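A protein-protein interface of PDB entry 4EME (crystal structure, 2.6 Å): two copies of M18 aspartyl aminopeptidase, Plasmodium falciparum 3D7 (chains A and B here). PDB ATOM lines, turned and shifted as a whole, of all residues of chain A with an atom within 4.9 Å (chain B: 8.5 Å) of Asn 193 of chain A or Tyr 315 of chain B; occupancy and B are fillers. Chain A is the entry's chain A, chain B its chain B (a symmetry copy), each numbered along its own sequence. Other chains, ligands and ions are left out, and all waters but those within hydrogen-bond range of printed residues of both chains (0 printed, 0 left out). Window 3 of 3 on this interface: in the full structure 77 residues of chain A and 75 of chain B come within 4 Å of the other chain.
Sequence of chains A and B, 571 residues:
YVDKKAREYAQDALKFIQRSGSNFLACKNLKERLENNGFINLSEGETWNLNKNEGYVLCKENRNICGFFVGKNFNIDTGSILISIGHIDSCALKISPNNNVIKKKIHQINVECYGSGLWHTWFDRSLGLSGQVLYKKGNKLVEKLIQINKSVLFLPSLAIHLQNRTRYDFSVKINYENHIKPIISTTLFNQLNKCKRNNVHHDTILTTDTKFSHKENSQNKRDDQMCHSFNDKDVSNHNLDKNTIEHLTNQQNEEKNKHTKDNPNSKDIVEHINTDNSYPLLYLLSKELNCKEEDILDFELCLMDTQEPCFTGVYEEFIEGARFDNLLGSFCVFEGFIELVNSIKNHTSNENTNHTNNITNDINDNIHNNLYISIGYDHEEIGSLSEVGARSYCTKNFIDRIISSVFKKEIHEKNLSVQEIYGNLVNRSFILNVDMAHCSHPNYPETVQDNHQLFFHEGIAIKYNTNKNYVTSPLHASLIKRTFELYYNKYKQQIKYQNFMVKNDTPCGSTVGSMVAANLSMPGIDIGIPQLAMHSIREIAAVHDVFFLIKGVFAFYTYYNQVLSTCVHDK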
ATOM      1  N   SER A 185     -18.822  18.656  14.494  1.00  0.00           N
ATOM      2  CA  SER A 185     -19.847  19.526  13.938  1.00  0.00           C
ATOM      3  C   SER A 185     -20.036  19.267  12.428  1.00  0.00           C
ATOM      4  O   SER A 185     -19.358  18.404  11.848  1.00  0.00           O
ATOM      5  CB  SER A 185     -19.492  20.995  14.196  1.00  0.00           C
ATOM      6  OG  SER A 185     -18.759  21.604  13.145  1.00  0.00           O
ATOM      7  N   PHE A 189     -23.397  24.246  10.507  1.00  0.00           N
ATOM      8  CA  PHE A 189     -23.408  24.842  11.834  1.00  0.00           C
ATOM      9  C   PHE A 189     -22.130  25.588  12.160  1.00  0.00           C
ATOM     10  O   PHE A 189     -22.207  26.609  12.854  1.00  0.00           O
ATOM     11  CB  PHE A 189     -23.802  23.838  12.916  1.00  0.00           C
ATOM     12  CG  PHE A 189     -25.299  23.692  13.034  1.00  0.00           C
ATOM     13  CD1 PHE A 189     -26.049  23.142  11.994  1.00  0.00           C
ATOM     14  CD2 PHE A 189     -25.967  24.121  14.174  1.00  0.00           C
ATOM     15  CE1 PHE A 189     -27.431  23.037  12.089  1.00  0.00           C
ATOM     16  CE2 PHE A 189     -27.352  23.985  14.279  1.00  0.00           C
ATOM     17  CZ  PHE A 189     -28.071  23.444  13.234  1.00  0.00           C
ATOM     18  N   ASN A 190     -20.970  25.143  11.616  1.00  0.00           N
ATOM     19  CA  ASN A 190     -19.717  25.876  11.823  1.00  0.00           C
ATOM     20  C   ASN A 190     -19.782  27.248  11.134  1.00  0.00           C
ATOM     21  O   ASN A 190     -19.362  28.245  11.719  1.00  0.00           O
ATOM     22  CB  ASN A 190     -18.496  25.083  11.357  1.00  0.00           C
ATOM     23  CG  ASN A 190     -17.212  25.684  11.849  1.00  0.00           C
ATOM     24  OD1 ASN A 190     -16.930  25.702  13.047  1.00  0.00           O
ATOM     25  ND2 ASN A 190     -16.419  26.218  10.944  1.00  0.00           N
ATOM     26  N   GLN A 191     -20.361  27.291   9.922  1.00  0.00           N
ATOM     27  CA  GLN A 191     -20.545  28.504   9.138  1.00  0.00           C
ATOM     28  C   GLN A 191     -21.579  29.427   9.740  1.00  0.00           C
ATOM     29  O   GLN A 191     -21.373  30.637   9.715  1.00  0.00           O
ATOM     30  CB  GLN A 191     -20.884  28.183   7.680  1.00  0.00           C
ATOM     31  CG  GLN A 191     -19.844  28.709   6.696  1.00  0.00           C
ATOM     32  CD  GLN A 191     -18.529  27.965   6.777  1.00  0.00           C
ATOM     33  OE1 GLN A 191     -17.569  28.419   7.413  1.00  0.00           O
ATOM     34  NE2 GLN A 191     -18.461  26.805   6.133  1.00  0.00           N
ATOM     35  N   LEU A 192     -22.682  28.885  10.283  1.00  0.00           N
ATOM     36  CA  LEU A 192     -23.715  29.732  10.886  1.00  0.00           C
ATOM     37  C   LEU A 192     -23.174  30.412  12.129  1.00  0.00           C
ATOM     38  O   LEU A 192     -23.324  31.625  12.266  1.00  0.00           O
ATOM     39  CB  LEU A 192     -25.018  28.961  11.216  1.00  0.00           C
ATOM     40  CG  LEU A 192     -25.859  28.409  10.047  1.00  0.00           C
ATOM     41  CD1 LEU A 192     -26.862  27.393  10.538  1.00  0.00           C
ATOM     42  CD2 LEU A 192     -26.603  29.506   9.316  1.00  0.00           C
ATOM     43  N   ASN A 193     -22.496  29.645  12.996  1.00  0.00           N
ATOM     44  CA  ASN A 193     -21.943  30.127  14.251  1.00  0.00           C
ATOM     45  C   ASN A 193     -20.934  31.233  14.152  1.00  0.00           C
ATOM     46  O   ASN A 193     -21.040  32.188  14.921  1.00  0.00           O
ATOM     47  CB  ASN A 193     -21.514  28.998  15.164  1.00  0.00           C
ATOM     48  CG  ASN A 193     -22.672  28.477  15.983  1.00  0.00           C
ATOM     49  OD1 ASN A 193     -22.753  28.704  17.200  1.00  0.00           O
ATOM     50  ND2 ASN A 193     -23.621  27.807  15.326  1.00  0.00           N
ATOM     51  N   LYS A 194     -19.992  31.160  13.198  1.00  0.00           N
ATOM     52  CA  LYS A 194     -19.043  32.265  13.034  1.00  0.00           C
ATOM     53  C   LYS A 194     -19.712  33.490  12.377  1.00  0.00           C
ATOM     54  O   LYS A 194     -19.355  34.626  12.701  1.00  0.00           O
ATOM     55  CB  LYS A 194     -17.715  31.849  12.383  1.00  0.00           C
ATOM     56  CG  LYS A 194     -17.816  31.133  11.041  1.00  0.00           C
ATOM     57  CD  LYS A 194     -16.437  30.942  10.396  1.00  0.00           C
ATOM     58  CE  LYS A 194     -15.606  29.853  11.030  1.00  0.00           C
ATOM     59  NZ  LYS A 194     -14.225  29.832  10.490  1.00  0.00           N
ATOM     60  N   CYS A 195     -20.761  33.248  11.547  1.00  0.00           N
ATOM     61  CA  CYS A 195     -21.586  34.279  10.899  1.00  0.00           C
ATOM     62  C   CYS A 195     -22.536  34.966  11.921  1.00  0.00           C
ATOM     63  O   CYS A 195     -23.063  36.049  11.647  1.00  0.00           O
ATOM     64  CB  CYS A 195     -22.362  33.688   9.722  1.00  0.00           C
ATOM     65  SG  CYS A 195     -22.476  34.781   8.281  1.00  0.00           S
ATOM     66  N   LYS A 196     -22.748  34.324  13.091  1.00  0.00           N
ATOM     67  CA  LYS A 196     -23.571  34.847  14.181  1.00  0.00           C
ATOM     68  C   LYS A 196     -22.694  35.589  15.199  1.00  0.00           C
ATOM     69  O   LYS A 196     -21.475  35.688  15.030  1.00  0.00           O
ATOM     70  CB  LYS A 196     -24.348  33.714  14.867  1.00  0.00           C
ATOM     71  N   TYR A 279     -11.576  24.324  13.753  1.00  0.00           N
ATOM     72  CA  TYR A 279     -12.214  25.553  14.238  1.00  0.00           C
ATOM     73  C   TYR A 279     -13.282  25.276  15.298  1.00  0.00           C
ATOM     74  O   TYR A 279     -13.196  25.918  16.353  1.00  0.00           O
ATOM     75  CB  TYR A 279     -12.724  26.508  13.145  1.00  0.00           C
ATOM     76  CG  TYR A 279     -13.268  27.783  13.759  1.00  0.00           C
ATOM     77  CD1 TYR A 279     -12.410  28.769  14.252  1.00  0.00           C
ATOM     78  CD2 TYR A 279     -14.635  27.945  13.975  1.00  0.00           C
ATOM     79  CE1 TYR A 279     -12.903  29.895  14.912  1.00  0.00           C
ATOM     80  CE2 TYR A 279     -15.137  29.063  14.640  1.00  0.00           C
ATOM     81  CZ  TYR A 279     -14.270  30.046  15.086  1.00  0.00           C
ATOM     82  OH  TYR A 279     -14.798  31.158  15.694  1.00  0.00           O
ATOM     83  N   PRO A 280     -14.248  24.324  15.102  1.00  0.00           N
ATOM     84  CA  PRO A 280     -15.218  24.052  16.188  1.00  0.00           C
ATOM     85  C   PRO A 280     -14.539  23.680  17.513  1.00  0.00           C
ATOM     86  O   PRO A 280     -15.081  23.986  18.574  1.00  0.00           O
ATOM     87  CB  PRO A 280     -16.074  22.905  15.650  1.00  0.00           C
ATOM     88  CG  PRO A 280     -15.809  22.846  14.188  1.00  0.00           C
ATOM     89  CD  PRO A 280     -14.501  23.473  13.913  1.00  0.00           C
ATOM     90  N   TYR A 283     -13.241  26.939  19.131  1.00  0.00           N
ATOM     91  CA  TYR A 283     -14.448  27.583  19.622  1.00  0.00           C
ATOM     92  C   TYR A 283     -14.839  26.977  20.979  1.00  0.00           C
ATOM     93  O   TYR A 283     -15.240  27.714  21.874  1.00  0.00           O
ATOM     94  CB  TYR A 283     -15.597  27.420  18.610  1.00  0.00           C
ATOM     95  CG  TYR A 283     -16.916  27.973  19.104  1.00  0.00           C
ATOM     96  CD1 TYR A 283     -17.262  29.300  18.886  1.00  0.00           C
ATOM     97  CD2 TYR A 283     -17.816  27.170  19.797  1.00  0.00           C
ATOM     98  CE1 TYR A 283     -18.465  29.822  19.362  1.00  0.00           C
ATOM     99  CE2 TYR A 283     -19.015  27.681  20.288  1.00  0.00           C
ATOM    100  CZ  TYR A 283     -19.338  29.009  20.065  1.00  0.00           C
ATOM    101  OH  TYR A 283     -20.542  29.508  20.512  1.00  0.00           O
ATOM    102  N   ASP B   3     -35.556  27.470  13.790  1.00  0.00           N
ATOM    103  CA  ASP B   3     -34.442  26.960  14.599  1.00  0.00           C
ATOM    104  C   ASP B   3     -34.845  26.655  16.045  1.00  0.00           C
ATOM    105  O   ASP B   3     -34.422  25.630  16.595  1.00  0.00           O
ATOM    106  CB  ASP B   3     -33.231  27.901  14.531  1.00  0.00           C
ATOM    107  CG  ASP B   3     -32.328  27.587  13.354  1.00  0.00           C
ATOM    108  OD1 ASP B   3     -31.366  26.795  13.536  1.00  0.00           O
ATOM    109  OD2 ASP B   3     -32.606  28.090  12.241  1.00  0.00           O
ATOM    110  N   ARG B   7     -35.211  22.598  17.672  1.00  0.00           N
ATOM    111  CA  ARG B   7     -34.613  22.214  18.937  1.00  0.00           C
ATOM    112  C   ARG B   7     -35.705  21.722  19.919  1.00  0.00           C
ATOM    113  O   ARG B   7     -35.474  20.773  20.665  1.00  0.00           O
ATOM    114  CB  ARG B   7     -33.775  23.388  19.477  1.00  0.00           C
ATOM    115  CG  ARG B   7     -33.467  23.360  20.980  1.00  0.00           C
ATOM    116  CD  ARG B   7     -32.078  22.859  21.298  1.00  0.00           C
ATOM    117  NE  ARG B   7     -31.860  22.798  22.744  1.00  0.00           N
ATOM    118  CZ  ARG B   7     -30.707  22.482  23.317  1.00  0.00           C
ATOM    119  NH1 ARG B   7     -29.641  22.204  22.576  1.00  0.00           N
ATOM    120  NH2 ARG B   7     -30.606  22.452  24.642  1.00  0.00           N
ATOM    121  N   PHE B 311     -28.283  15.863  23.453  1.00  0.00           N
ATOM    122  CA  PHE B 311     -27.724  16.596  22.330  1.00  0.00           C
ATOM    123  C   PHE B 311     -26.185  16.425  22.327  1.00  0.00           C
ATOM    124  O   PHE B 311     -25.589  16.237  23.393  1.00  0.00           O
ATOM    125  CB  PHE B 311     -28.092  18.094  22.393  1.00  0.00           C
ATOM    126  CG  PHE B 311     -29.540  18.409  22.101  1.00  0.00           C
ATOM    127  CD1 PHE B 311     -30.494  18.387  23.114  1.00  0.00           C
ATOM    128  CD2 PHE B 311     -29.946  18.776  20.822  1.00  0.00           C
ATOM    129  CE1 PHE B 311     -31.828  18.699  22.847  1.00  0.00           C
ATOM    130  CE2 PHE B 311     -31.282  19.099  20.562  1.00  0.00           C
ATOM    131  CZ  PHE B 311     -32.213  19.053  21.576  1.00  0.00           C
ATOM    132  N   THR B 312     -25.549  16.476  21.132  1.00  0.00           N
ATOM    133  CA  THR B 312     -24.091  16.400  20.996  1.00  0.00           C
ATOM    134  C   THR B 312     -23.550  17.395  19.977  1.00  0.00           C
ATOM    135  O   THR B 312     -24.312  18.024  19.249  1.00  0.00           O
ATOM    136  CB  THR B 312     -23.543  14.950  20.942  1.00  0.00           C
ATOM    137  OG1 THR B 312     -22.121  14.973  21.078  1.00  0.00           O
ATOM    138  CG2 THR B 312     -23.927  14.195  19.684  1.00  0.00           C
ATOM    139  N   GLY B 313     -22.235  17.541  19.940  1.00  0.00           N
ATOM    140  CA  GLY B 313     -21.595  18.494  19.044  1.00  0.00           C
ATOM    141  C   GLY B 313     -21.437  19.824  19.741  1.00  0.00           C
ATOM    142  O   GLY B 313     -22.251  20.196  20.595  1.00  0.00           O
ATOM    143  N   VAL B 314     -20.375  20.534  19.391  1.00  0.00           N
ATOM    144  CA  VAL B 314     -20.029  21.825  19.961  1.00  0.00           C
ATOM    145  C   VAL B 314     -21.206  22.794  19.862  1.00  0.00           C
ATOM    146  O   VAL B 314     -21.437  23.549  20.797  1.00  0.00           O
ATOM    147  CB  VAL B 314     -18.712  22.334  19.332  1.00  0.00           C
ATOM    148  CG1 VAL B 314     -18.531  23.828  19.494  1.00  0.00           C
ATOM    149  CG2 VAL B 314     -17.537  21.608  19.952  1.00  0.00           C
ATOM    150  N   TYR B 315     -21.990  22.708  18.774  1.00  0.00           N
ATOM    151  CA  TYR B 315     -23.136  23.569  18.532  1.00  0.00           C
ATOM    152  C   TYR B 315     -24.457  22.903  18.896  1.00  0.00           C
ATOM    153  O   TYR B 315     -25.518  23.409  18.509  1.00  0.00           O
ATOM    154  CB  TYR B 315     -23.126  24.051  17.069  1.00  0.00           C
ATOM    155  CG  TYR B 315     -21.786  24.593  16.607  1.00  0.00           C
ATOM    156  CD1 TYR B 315     -21.173  25.653  17.269  1.00  0.00           C
ATOM    157  CD2 TYR B 315     -21.131  24.046  15.506  1.00  0.00           C
ATOM    158  CE1 TYR B 315     -19.935  26.142  16.862  1.00  0.00           C
ATOM    159  CE2 TYR B 315     -19.893  24.531  15.085  1.00  0.00           C
ATOM    160  CZ  TYR B 315     -19.308  25.596  15.753  1.00  0.00           C
ATOM    161  OH  TYR B 315     -18.097  26.100  15.341  1.00  0.00           O
ATOM    162  N   GLU B 316     -24.407  21.768  19.639  1.00  0.00           N
ATOM    163  CA  GLU B 316     -25.575  20.970  20.058  1.00  0.00           C
ATOM    164  C   GLU B 316     -26.545  20.718  18.880  1.00  0.00           C
ATOM    165  O   GLU B 316     -27.771  20.794  19.023  1.00  0.00           O
ATOM    166  CB  GLU B 316     -26.287  21.647  21.225  1.00  0.00           C
ATOM    167  CG  GLU B 316     -25.514  21.625  22.529  1.00  0.00           C
ATOM    168  CD  GLU B 316     -26.230  22.384  23.625  1.00  0.00           C
ATOM    169  OE1 GLU B 316     -27.317  21.933  24.055  1.00  0.00           O
ATOM    170  OE2 GLU B 316     -25.721  23.455  24.025  1.00  0.00           O
ATOM    171  N   GLU B 317     -25.968  20.467  17.713  1.00  0.00           N
ATOM    172  CA  GLU B 317     -26.688  20.273  16.469  1.00  0.00           C
ATOM    173  C   GLU B 317     -27.058  18.828  16.240  1.00  0.00           C
ATOM    174  O   GLU B 317     -27.783  18.533  15.286  1.00  0.00           O
ATOM    175  CB  GLU B 317     -25.836  20.760  15.305  1.00  0.00           C
ATOM    176  CG  GLU B 317     -24.620  19.883  15.079  1.00  0.00           C
ATOM    177  CD  GLU B 317     -23.811  20.331  13.895  1.00  0.00           C
ATOM    178  OE1 GLU B 317     -24.310  20.202  12.755  1.00  0.00           O
ATOM    179  OE2 GLU B 317     -22.721  20.901  14.117  1.00  0.00           O
ATOM    180  N   PHE B 318     -26.493  17.926  17.042  1.00  0.00           N
ATOM    181  CA  PHE B 318     -26.786  16.503  16.925  1.00  0.00           C
ATOM    182  C   PHE B 318     -27.583  16.008  18.117  1.00  0.00           C
ATOM    183  O   PHE B 318     -27.496  16.565  19.215  1.00  0.00           O
ATOM    184  CB  PHE B 318     -25.504  15.663  16.791  1.00  0.00           C
ATOM    185  CG  PHE B 318     -24.560  16.058  15.688  1.00  0.00           C
ATOM    186  CD1 PHE B 318     -24.927  15.920  14.347  1.00  0.00           C
ATOM    187  CD2 PHE B 318     -23.289  16.548  15.980  1.00  0.00           C
ATOM    188  CE1 PHE B 318     -24.058  16.318  13.321  1.00  0.00           C
ATOM    189  CE2 PHE B 318     -22.409  16.904  14.954  1.00  0.00           C
ATOM    190  CZ  PHE B 318     -22.806  16.795  13.632  1.00  0.00           C
ATOM    191  N   HIS B 457     -28.844  17.706   8.295  1.00  0.00           N
ATOM    192  CA  HIS B 457     -29.536  19.007   8.146  1.00  0.00           C
ATOM    193  C   HIS B 457     -29.964  19.312   6.701  1.00  0.00           C
ATOM    194  O   HIS B 457     -30.594  20.344   6.462  1.00  0.00           O
ATOM    195  CB  HIS B 457     -28.767  20.195   8.774  1.00  0.00           C
ATOM    196  CG  HIS B 457     -28.200  19.937  10.132  1.00  0.00           C
ATOM    197  ND1 HIS B 457     -29.006  19.875  11.251  1.00  0.00           N
ATOM    198  CD2 HIS B 457     -26.910  19.787  10.516  1.00  0.00           C
ATOM    199  CE1 HIS B 457     -28.193  19.662  12.274  1.00  0.00           C
ATOM    200  NE2 HIS B 457     -26.921  19.601  11.883  1.00  0.00           N
ATOM    201  N   VAL B 543     -30.609  17.707  14.232  1.00  0.00           N
ATOM    202  CA  VAL B 543     -31.733  18.518  14.706  1.00  0.00           C
ATOM    203  C   VAL B 543     -32.641  19.071  13.599  1.00  0.00           C
ATOM    204  O   VAL B 543     -33.866  18.924  13.710  1.00  0.00           O
ATOM    205  CB  VAL B 543     -31.278  19.602  15.736  1.00  0.00           C
ATOM    206  CG1 VAL B 543     -32.436  20.507  16.165  1.00  0.00           C
ATOM    207  CG2 VAL B 543     -30.626  18.953  16.955  1.00  0.00           C
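OD1 of Asn 190 of chain A lies within hydrogen-bond range of OH of Tyr 315 of chain B (2.6 Å).
The backbone NH of Val 543 of chain B lies within hydrogen-bond range of the backbone carbonyl oxygen of Glu 317 of chain B (3.1 Å).
The backbone carbonyl oxygen (O) of Thr 312 of chain B is in hydrogen-bond range of the backbone NH (N) of Glu 317 of chain B (3.3 Å).
O of Phe 318 of chain B is in hydrogen-bond range of N of Thr 312 of chain B, at 2.7 Å.
O of Phe 189 of chain A lies within hydrogen-bond range of ND2 of Asn 193 of chain A, 3.1 Å away.
OE1 of Glu 317 of chain B lies within hydrogen-bond range of NE2 of His 457 of chain B.
Tyr 315 of chain B touches Ser 185 of chain A (CE2 to CB, 3.7 Å).
Glu 317 of chain B touches Ser 185 of chain A.
Ser 185 of chain A touches Phe 318 of chain B.
CB of Phe 189 of chain A touches CD2 of Tyr 315 of chain B, at 3.7 Å.
Phe 189 of chain A touches Glu 317 of chain B.
His 457 of chain B touches Phe 189 of chain A.
OD1 of Asn 193 of chain A touches CD1 of Tyr 315 of chain B, 3.4 Å away.
Pro 280 of chain A touches Val 314 of chain B (O to CG1, 3.6 Å).
Val 314 of chain B touches Tyr 283 of chain A (CG1 to CD2, 3.4 Å).
Tyr 315 of chain B touches Tyr 283 of chain A.
Asn 193 of chain A touches just one residue of chain B: Tyr 315.
Printed residues of chain B within 4 Å of Tyr 283 of chain A: Val 314 and Tyr 315.
Tyr 315 of chain B touches six residues of chain A.
Of the printed residues of chain A, Glu 317 of chain B touches Ser 185 (3.2 Å) and Phe 189 (3.4 Å).
Printed residues of chain A within 4 Å of Phe 318 of chain B: Ser 185.
Val 543 of chain B touches none of the printed residues of chain A.
The nearest residue of chain B that does not touch Asn 193 of chain A is Val 314 of chain B (6.4 Å).
The nearest residue of chain A that does not touch Tyr 315 of chain B is Tyr 279 of chain A (4.2 Å).
Along chain B the printed residues that touch a printed residue of chain A span positions 314 to 457.
Of the 12 printed residues of chain A, 6 touch a printed residue of chain B.
Hydrophobic or aromatic side chains of chain A that line the printed part of chain B: Phe 189, Pro 280 and Tyr 283.
Among the printed residues, 12 pairs touch across the chains.
Among the printed residues, no Asp or Glu carboxylate lies within 4 Å of a Lys or Arg side-chain nitrogen of the other chain.
No position is printed for both chains.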
